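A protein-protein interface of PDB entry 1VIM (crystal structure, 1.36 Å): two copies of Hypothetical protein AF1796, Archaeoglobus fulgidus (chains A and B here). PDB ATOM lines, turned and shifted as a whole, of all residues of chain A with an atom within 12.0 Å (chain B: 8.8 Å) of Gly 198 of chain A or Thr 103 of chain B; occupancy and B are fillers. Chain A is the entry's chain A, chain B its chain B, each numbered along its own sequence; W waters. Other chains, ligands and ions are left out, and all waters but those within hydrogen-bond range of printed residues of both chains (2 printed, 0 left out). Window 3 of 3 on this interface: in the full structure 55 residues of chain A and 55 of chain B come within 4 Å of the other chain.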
ATOM      1  N   GLU A 189      -9.061  39.745   2.355  1.00  0.00           N
ATOM      2  CA  GLU A 189      -9.513  39.365   3.684  1.00  0.00           C
ATOM      3  C   GLU A 189     -10.734  40.165   4.113  1.00  0.00           C
ATOM      4  O   GLU A 189     -11.624  39.641   4.786  1.00  0.00           O
ATOM      5  CB  GLU A 189      -8.363  39.545   4.672  1.00  0.00           C
ATOM      6  CG  GLU A 189      -8.415  38.699   5.931  1.00  0.00           C
ATOM      7  CD  GLU A 189      -7.132  38.838   6.744  1.00  0.00           C
ATOM      8  OE1 GLU A 189      -6.528  39.930   6.710  1.00  0.00           O
ATOM      9  OE2 GLU A 189      -6.708  37.851   7.389  1.00  0.00           O
ATOM     10  N   ARG A 191     -13.209  41.093   2.359  1.00  0.00           N
ATOM     11  CA  ARG A 191     -14.413  40.615   1.680  1.00  0.00           C
ATOM     12  C   ARG A 191     -14.737  39.159   1.960  1.00  0.00           C
ATOM     13  O   ARG A 191     -15.856  38.714   1.679  1.00  0.00           O
ATOM     14  CB  ARG A 191     -14.265  40.792   0.165  1.00  0.00           C
ATOM     15  CG  ARG A 191     -14.124  42.244  -0.294  1.00  0.00           C
ATOM     16  CD  ARG A 191     -14.376  42.413  -1.792  1.00  0.00           C
ATOM     17  NE  ARG A 191     -14.116  43.776  -2.255  1.00  0.00           N
ATOM     18  CZ  ARG A 191     -12.941  44.229  -2.696  1.00  0.00           C
ATOM     19  NH1 ARG A 191     -11.859  43.451  -2.724  1.00  0.00           N
ATOM     20  NH2 ARG A 191     -12.848  45.489  -3.105  1.00  0.00           N
ATOM     21  N   HIS A 192     -13.798  38.379   2.471  1.00  0.00           N
ATOM     22  CA  HIS A 192     -14.083  36.951   2.606  1.00  0.00           C
ATOM     23  C   HIS A 192     -15.088  36.628   3.703  1.00  0.00           C
ATOM     24  O   HIS A 192     -15.162  37.301   4.752  1.00  0.00           O
ATOM     25  CB  HIS A 192     -12.796  36.134   2.654  1.00  0.00           C
ATOM     26  CG  HIS A 192     -12.121  36.101   3.976  1.00  0.00           C
ATOM     27  ND1 HIS A 192     -12.385  36.998   4.986  1.00  0.00           N
ATOM     28  CD2 HIS A 192     -11.148  35.283   4.445  1.00  0.00           C
ATOM     29  CE1 HIS A 192     -11.623  36.719   6.031  1.00  0.00           C
ATOM     30  NE2 HIS A 192     -10.863  35.686   5.728  1.00  0.00           N
ATOM     31  N   ALA A 193     -15.897  35.605   3.446  1.00  0.00           N
ATOM     32  CA  ALA A 193     -16.907  35.160   4.400  1.00  0.00           C
ATOM     33  C   ALA A 193     -16.250  34.632   5.661  1.00  0.00           C
ATOM     34  O   ALA A 193     -15.207  33.985   5.591  1.00  0.00           O
ATOM     35  CB  ALA A 193     -17.758  34.054   3.777  1.00  0.00           C
ATOM     36  N   VAL A 194     -16.884  34.886   6.797  1.00  0.00           N
ATOM     37  CA  VAL A 194     -16.360  34.487   8.096  1.00  0.00           C
ATOM     38  C   VAL A 194     -17.272  33.628   8.950  1.00  0.00           C
ATOM     39  O   VAL A 194     -16.829  33.079   9.977  1.00  0.00           O
ATOM     40  CB  VAL A 194     -15.919  35.726   8.945  1.00  0.00           C
ATOM     41  CG1 VAL A 194     -14.841  36.509   8.220  1.00  0.00           C
ATOM     42  CG2 VAL A 194     -17.107  36.591   9.309  1.00  0.00           C
ATOM     43  N   LEU A 195     -18.545  33.500   8.580  1.00  0.00           N
ATOM     44  CA  LEU A 195     -19.497  32.850   9.480  1.00  0.00           C
ATOM     45  C   LEU A 195     -19.191  31.368   9.761  1.00  0.00           C
ATOM     46  O   LEU A 195     -19.249  30.941  10.923  1.00  0.00           O
ATOM     47  CB  LEU A 195     -20.924  33.061   9.012  1.00  0.00           C
ATOM     48  CG  LEU A 195     -21.443  34.489   9.202  1.00  0.00           C
ATOM     49  CD1 LEU A 195     -22.765  34.603   8.465  1.00  0.00           C
ATOM     50  CD2 LEU A 195     -21.620  34.812  10.662  1.00  0.00           C
ATOM     51  N   GLU A 196     -18.782  30.632   8.724  1.00  0.00           N
ATOM     52  CA  GLU A 196     -18.462  29.202   8.892  1.00  0.00           C
ATOM     53  C   GLU A 196     -16.995  28.905   9.191  1.00  0.00           C
ATOM     54  O   GLU A 196     -16.648  27.757   9.519  1.00  0.00           O
ATOM     55  CB  GLU A 196     -18.909  28.409   7.656  1.00  0.00           C
ATOM     56  CG  GLU A 196     -20.415  28.508   7.468  1.00  0.00           C
ATOM     57  CD  GLU A 196     -21.040  27.531   6.492  1.00  0.00           C
ATOM     58  OE1 GLU A 196     -20.332  26.702   5.875  1.00  0.00           O
ATOM     59  OE2 GLU A 196     -22.279  27.606   6.359  1.00  0.00           O
ATOM     60  N   GLU A 197     -16.121  29.889   9.043  1.00  0.00           N
ATOM     61  CA  GLU A 197     -14.692  29.649   9.244  1.00  0.00           C
ATOM     62  C   GLU A 197     -14.169  30.250  10.543  1.00  0.00           C
ATOM     63  O   GLU A 197     -13.291  29.663  11.190  1.00  0.00           O
ATOM     64  CB  GLU A 197     -13.897  30.164   8.058  1.00  0.00           C
ATOM     65  CG  GLU A 197     -14.146  29.328   6.806  1.00  0.00           C
ATOM     66  CD  GLU A 197     -13.393  29.832   5.589  1.00  0.00           C
ATOM     67  OE1 GLU A 197     -12.732  30.902   5.663  1.00  0.00           O
ATOM     68  OE2 GLU A 197     -13.477  29.170   4.541  1.00  0.00           O
ATOM     69  N   GLY A 198     -14.714  31.403  10.919  1.00  0.00           N
ATOM     70  CA  GLY A 198     -14.351  32.078  12.166  1.00  0.00           C
ATOM     71  C   GLY A 198     -13.118  32.946  12.050  1.00  0.00           C
ATOM     72  O   GLY A 198     -12.598  33.449  13.067  1.00  0.00           O
ATOM     73  N   GLY A 199     -12.638  33.116  10.821  1.00  0.00           N
ATOM     74  CA  GLY A 199     -11.462  33.928  10.539  1.00  0.00           C
ATOM     75  C   GLY A 199     -10.189  33.349  11.122  1.00  0.00           C
ATOM     76  O   GLY A 199      -9.324  32.848  10.395  1.00  0.00           O
ATOM     77  N   ILE B  53     -15.775  16.720   4.901  1.00  0.00           N
ATOM     78  CA  ILE B  53     -16.182  18.097   5.181  1.00  0.00           C
ATOM     79  C   ILE B  53     -15.041  19.072   5.020  1.00  0.00           C
ATOM     80  O   ILE B  53     -13.924  18.771   5.373  1.00  0.00           O
ATOM     81  CB  ILE B  53     -16.778  18.217   6.619  1.00  0.00           C
ATOM     82  CG1 ILE B  53     -17.349  19.612   6.863  1.00  0.00           C
ATOM     83  CG2 ILE B  53     -15.730  17.829   7.703  1.00  0.00           C
ATOM     84  CD1 ILE B  53     -18.003  19.735   8.189  1.00  0.00           C
ATOM     85  N   ALA B  55     -14.844  23.745   4.859  1.00  0.00           N
ATOM     86  CA  ALA B  55     -15.543  25.025   4.724  1.00  0.00           C
ATOM     87  C   ALA B  55     -15.013  25.819   3.545  1.00  0.00           C
ATOM     88  O   ALA B  55     -13.831  25.804   3.258  1.00  0.00           O
ATOM     89  CB  ALA B  55     -15.385  25.858   6.017  1.00  0.00           C
ATOM     90  N   SER B  97      -8.919  21.258   6.640  1.00  0.00           N
ATOM     91  CA  SER B  97      -8.826  22.609   7.202  1.00  0.00           C
ATOM     92  C   SER B  97      -7.352  22.981   7.272  1.00  0.00           C
ATOM     93  O   SER B  97      -6.583  22.350   7.992  1.00  0.00           O
ATOM     94  CB  SER B  97      -9.426  22.668   8.614  1.00  0.00           C
ATOM     95  OG  SER B  97      -9.040  23.891   9.258  1.00  0.00           O
ATOM     96  N   SER B  99      -5.810  25.609   8.626  1.00  0.00           N
ATOM     97  CA  SER B  99      -5.382  26.010   9.947  1.00  0.00           C
ATOM     98  C   SER B  99      -5.623  24.963  11.010  1.00  0.00           C
ATOM     99  O   SER B  99      -5.020  25.013  12.100  1.00  0.00           O
ATOM    100  CB  SER B  99      -6.149  27.266  10.347  1.00  0.00           C
ATOM    101  OG  SER B  99      -7.529  26.970  10.535  1.00  0.00           O
ATOM    102  N   GLY B 100      -6.567  24.058  10.747  1.00  0.00           N
ATOM    103  CA  GLY B 100      -7.017  23.166  11.796  1.00  0.00           C
ATOM    104  C   GLY B 100      -7.845  23.832  12.875  1.00  0.00           C
ATOM    105  O   GLY B 100      -8.154  23.197  13.887  1.00  0.00           O
ATOM    106  N   GLU B 101      -8.247  25.082  12.637  1.00  0.00           N
ATOM    107  CA  GLU B 101      -9.043  25.840  13.602  1.00  0.00           C
ATOM    108  C   GLU B 101     -10.365  26.324  13.029  1.00  0.00           C
ATOM    109  O   GLU B 101     -11.132  26.975  13.735  1.00  0.00           O
ATOM    110  CB  GLU B 101      -8.245  27.031  14.160  1.00  0.00           C
ATOM    111  CG  GLU B 101      -6.934  26.624  14.806  1.00  0.00           C
ATOM    112  CD  GLU B 101      -7.090  25.786  16.070  1.00  0.00           C
ATOM    113  OE1 GLU B 101      -8.185  25.759  16.656  1.00  0.00           O
ATOM    114  OE2 GLU B 101      -6.113  25.146  16.482  1.00  0.00           O
ATOM    115  N   THR B 102     -10.644  25.980  11.772  1.00  0.00           N
ATOM    116  CA  THR B 102     -11.901  26.350  11.107  1.00  0.00           C
ATOM    117  C   THR B 102     -13.086  25.969  11.978  1.00  0.00           C
ATOM    118  O   THR B 102     -13.257  24.797  12.299  1.00  0.00           O
ATOM    119  CB  THR B 102     -11.988  25.576   9.803  1.00  0.00           C
ATOM    120  OG1 THR B 102     -10.839  25.855   9.008  1.00  0.00           O
ATOM    121  CG2 THR B 102     -13.224  25.999   8.958  1.00  0.00           C
ATOM    122  N   THR B 103     -13.938  26.932  12.339  1.00  0.00           N
ATOM    123  CA  THR B 103     -14.916  26.704  13.403  1.00  0.00           C
ATOM    124  C   THR B 103     -15.940  25.611  13.068  1.00  0.00           C
ATOM    125  O   THR B 103     -16.166  24.692  13.864  1.00  0.00           O
ATOM    126  CB  THR B 103     -15.640  28.017  13.733  1.00  0.00           C
ATOM    127  OG1 THR B 103     -16.041  28.623  12.496  1.00  0.00           O
ATOM    128  CG2 THR B 103     -14.646  28.977  14.313  1.00  0.00           C
ATOM    129  N   SER B 104     -16.534  25.690  11.880  1.00  0.00           N
ATOM    130  CA  SER B 104     -17.561  24.720  11.515  1.00  0.00           C
ATOM    131  C   SER B 104     -16.979  23.302  11.462  1.00  0.00           C
ATOM    132  O   SER B 104     -17.611  22.351  11.926  1.00  0.00           O
ATOM    133  CB  SER B 104     -18.210  25.085  10.174  1.00  0.00           C
ATOM    134  OG  SER B 104     -17.264  25.122   9.121  1.00  0.00           O
ATOM    135  N   VAL B 105     -15.749  23.178  10.983  1.00  0.00           N
ATOM    136  CA  VAL B 105     -15.146  21.864  10.788  1.00  0.00           C
ATOM    137  C   VAL B 105     -14.752  21.269  12.135  1.00  0.00           C
ATOM    138  O   VAL B 105     -14.955  20.089  12.366  1.00  0.00           O
ATOM    139  CB  VAL B 105     -13.943  21.955   9.798  1.00  0.00           C
ATOM    140  CG1 VAL B 105     -13.195  20.637   9.734  1.00  0.00           C
ATOM    141  CG2 VAL B 105     -14.435  22.332   8.403  1.00  0.00           C
ATOM    142  N   VAL B 106     -14.230  22.106  13.032  1.00  0.00           N
ATOM    143  CA  VAL B 106     -13.901  21.647  14.373  1.00  0.00           C
ATOM    144  C   VAL B 106     -15.155  21.229  15.141  1.00  0.00           C
ATOM    145  O   VAL B 106     -15.173  20.162  15.762  1.00  0.00           O
ATOM    146  CB  VAL B 106     -13.125  22.726  15.144  1.00  0.00           C
ATOM    147  CG1 VAL B 106     -13.059  22.391  16.632  1.00  0.00           C
ATOM    148  CG2 VAL B 106     -11.719  22.858  14.564  1.00  0.00           C
ATOM    149  N   ASN B 107     -16.211  22.030  15.052  1.00  0.00           N
ATOM    150  CA  ASN B 107     -17.468  21.700  15.751  1.00  0.00           C
ATOM    151  C   ASN B 107     -18.085  20.384  15.246  1.00  0.00           C
ATOM    152  O   ASN B 107     -18.508  19.536  16.033  1.00  0.00           O
ATOM    153  CB  ASN B 107     -18.491  22.840  15.600  1.00  0.00           C
ATOM    154  CG  ASN B 107     -18.106  24.095  16.366  1.00  0.00           C
ATOM    155  OD1 ASN B 107     -17.314  24.043  17.280  1.00  0.00           O
ATOM    156  ND2 ASN B 107     -18.677  25.220  15.969  1.00  0.00           N
ATOM    157  N   ILE B 108     -18.128  20.229  13.921  1.00  0.00           N
ATOM    158  CA  ILE B 108     -18.699  19.024  13.326  1.00  0.00           C
ATOM    159  C   ILE B 108     -17.849  17.805  13.685  1.00  0.00           C
ATOM    160  O   ILE B 108     -18.367  16.717  13.993  1.00  0.00           O
ATOM    161  CB  ILE B 108     -18.831  19.197  11.791  1.00  0.00           C
ATOM    162  CG1 ILE B 108     -20.015  20.108  11.477  1.00  0.00           C
ATOM    163  CG2 ILE B 108     -18.973  17.824  11.087  1.00  0.00           C
ATOM    164  CD1 ILE B 108     -19.946  20.768  10.139  1.00  0.00           C
ATOM    165  N   SER B 109     -16.530  17.995  13.656  1.00  0.00           N
ATOM    166  CA  SER B 109     -15.636  16.859  13.911  1.00  0.00           C
ATOM    167  C   SER B 109     -15.743  16.399  15.365  1.00  0.00           C
ATOM    168  O   SER B 109     -15.682  15.198  15.654  1.00  0.00           O
ATOM    169  CB  SER B 109     -14.180  17.189  13.565  1.00  0.00           C
ATOM    170  OG  SER B 109     -14.069  17.433  12.178  1.00  0.00           O
ATOM    171  N   LYS B 110     -15.868  17.358  16.288  1.00  0.00           N
ATOM    172  CA  LYS B 110     -16.076  17.001  17.689  1.00  0.00           C
ATOM    173  C   LYS B 110     -17.368  16.189  17.860  1.00  0.00           C
ATOM    174  O   LYS B 110     -17.364  15.193  18.584  1.00  0.00           O
ATOM    175  CB  LYS B 110     -16.058  18.259  18.587  1.00  0.00           C
ATOM    176  CG  LYS B 110     -16.406  17.986  20.084  1.00  0.00           C
ATOM    177  CD  LYS B 110     -15.506  16.919  20.746  1.00  0.00           C
ATOM    178  CE  LYS B 110     -15.712  16.822  22.277  1.00  0.00           C
ATOM    179  NZ  LYS B 110     -17.114  17.036  22.726  1.00  0.00           N
ATOM    180  N   SER B 129      -6.477  22.370  16.884  1.00  0.00           N
ATOM    181  CA  SER B 129      -7.677  21.760  17.480  1.00  0.00           C
ATOM    182  C   SER B 129      -8.156  20.530  16.682  1.00  0.00           C
ATOM    183  O   SER B 129      -8.463  19.477  17.262  1.00  0.00           O
ATOM    184  CB  SER B 129      -8.823  22.761  17.550  1.00  0.00           C
ATOM    185  OG  SER B 129      -8.482  23.844  18.394  1.00  0.00           O
ATOM    186  N   LEU B 130      -8.207  20.667  15.356  1.00  0.00           N
ATOM    187  CA  LEU B 130      -8.697  19.578  14.524  1.00  0.00           C
ATOM    188  C   LEU B 130      -7.784  18.374  14.593  1.00  0.00           C
ATOM    189  O   LEU B 130      -8.248  17.231  14.765  1.00  0.00           O
ATOM    190  CB  LEU B 130      -8.829  20.020  13.065  1.00  0.00           C
ATOM    191  CG  LEU B 130      -9.479  18.955  12.180  1.00  0.00           C
ATOM    192  CD1 LEU B 130     -10.907  18.609  12.598  1.00  0.00           C
ATOM    193  CD2 LEU B 130      -9.409  19.435  10.732  1.00  0.00           C
ATOM    194  N   MET B 133      -7.934  16.095  17.776  1.00  0.00           N
ATOM    195  CA  MET B 133      -9.072  15.179  17.842  1.00  0.00           C
ATOM    196  C   MET B 133      -8.937  13.961  16.926  1.00  0.00           C
ATOM    197  O   MET B 133      -9.692  12.996  17.052  1.00  0.00           O
ATOM    198  CB  MET B 133     -10.363  15.915  17.459  1.00  0.00           C
ATOM    199  CG  MET B 133     -10.833  16.915  18.491  1.00  0.00           C
ATOM    200  SD  MET B 133     -12.481  17.477  18.100  1.00  0.00           S
ATOM    201  CE  MET B 133     -12.070  18.466  16.699  1.00  0.00           C
HETATM  202  O   HOH W   1     -18.538  24.503   6.663  1.00  0.00           O
HETATM  203  O   HOH W   2     -17.239  31.136  12.847  1.00  0.00           O
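ND2 of Asn 107 of chain B sits close to O of Thr 103 of chain B (3.3 Å). OG1 of Thr 102 of chain B lies within hydrogen-bond range of OG of Ser 97 of chain B (2.7 Å). N of Thr 102 of chain B sits at hydrogen-bond distance from OG of Ser 99 of chain B, 3.5 Å away.
N of Gly 198 of chain A is in hydrogen-bond range of OG1 of Thr 103 of chain B. O of Glu 196 of chain A sits at hydrogen-bond distance from OG of Ser 104 of chain B (2.7 Å). O of Glu 197 of chain A is in hydrogen-bond range of N of Thr 103 of chain B, at 3.0 Å. O of Glu 196 of chain A is in hydrogen-bond range of OG1 of Thr 103 of chain B, at 3.2 Å.
No position is printed for both chains. Of the 7 pairs that touch across the chains among the printed residues, none has its exchanged pair printed and touching as well.
Along chain A the printed residues that touch a printed residue of chain B span positions 196 to 198. Among the printed residues, 7 pairs touch across the chains. Among the printed residues, no Asp or Glu carboxylate lies within 4 Å of a Lys or Arg side-chain nitrogen of the other chain.
Gly 198 of chain A touches just one residue of chain B: Thr 103 (3.5 Å). Thr 103 of chain B touches just these residues of chain A: Glu 196 (3.2 Å), Glu 197 (3.0 Å) and Gly 198 (3.5 Å). Thr 102 of chain B touches two residues of chain A. Ser 104 of chain B touches just one residue of chain A: Glu 196. No residue of chain A comes within 4 Å of Val 106 of chain B. No residue of chain A comes within 4 Å of Asn 107 of chain B. Printed residues of chain B within 4 Å of Glu 196 of chain A: Thr 102, Thr 103 and Ser 104. Of the printed residues of chain A, Ala 55 of chain B touches Glu 197. Of the printed residues of chain B, Glu 197 of chain A touches Ala 55, Thr 102 and Thr 103. Ser 109 of chain B touches none of the printed residues of chain A. Arg 191 of chain A touches none of the printed residues of chain B. The nearest residue of chain B that does not touch Gly 198 of chain A is Thr 102 of chain B (5.8 Å). The nearest residue of chain A that does not touch Thr 103 of chain B is Leu 195 of chain A (4.3 Å).
Water W2 lies within hydrogen-bond range of the backbone carbonyl oxygen of Leu 195 of chain A, the side-chain hydroxyl of Thr 103 of chain B, the backbone NH of Gly 198 of chain A and the backbone carbonyl oxygen of Val 194 of chain A. Water W1 bridges OG of Ser 104 of chain B (2.8 Å) and OE1 of Glu 196 of chain A (2.9 Å).
Among the printed residues, merely in contact across the chains: Glu 196 of chain A with Thr 102 of chain B (3.9 Å), Glu 197 of chain A with Ala 55 of chain B (3.6 Å) and Glu 197 of chain A with Thr 102 of chain B (3.6 Å).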
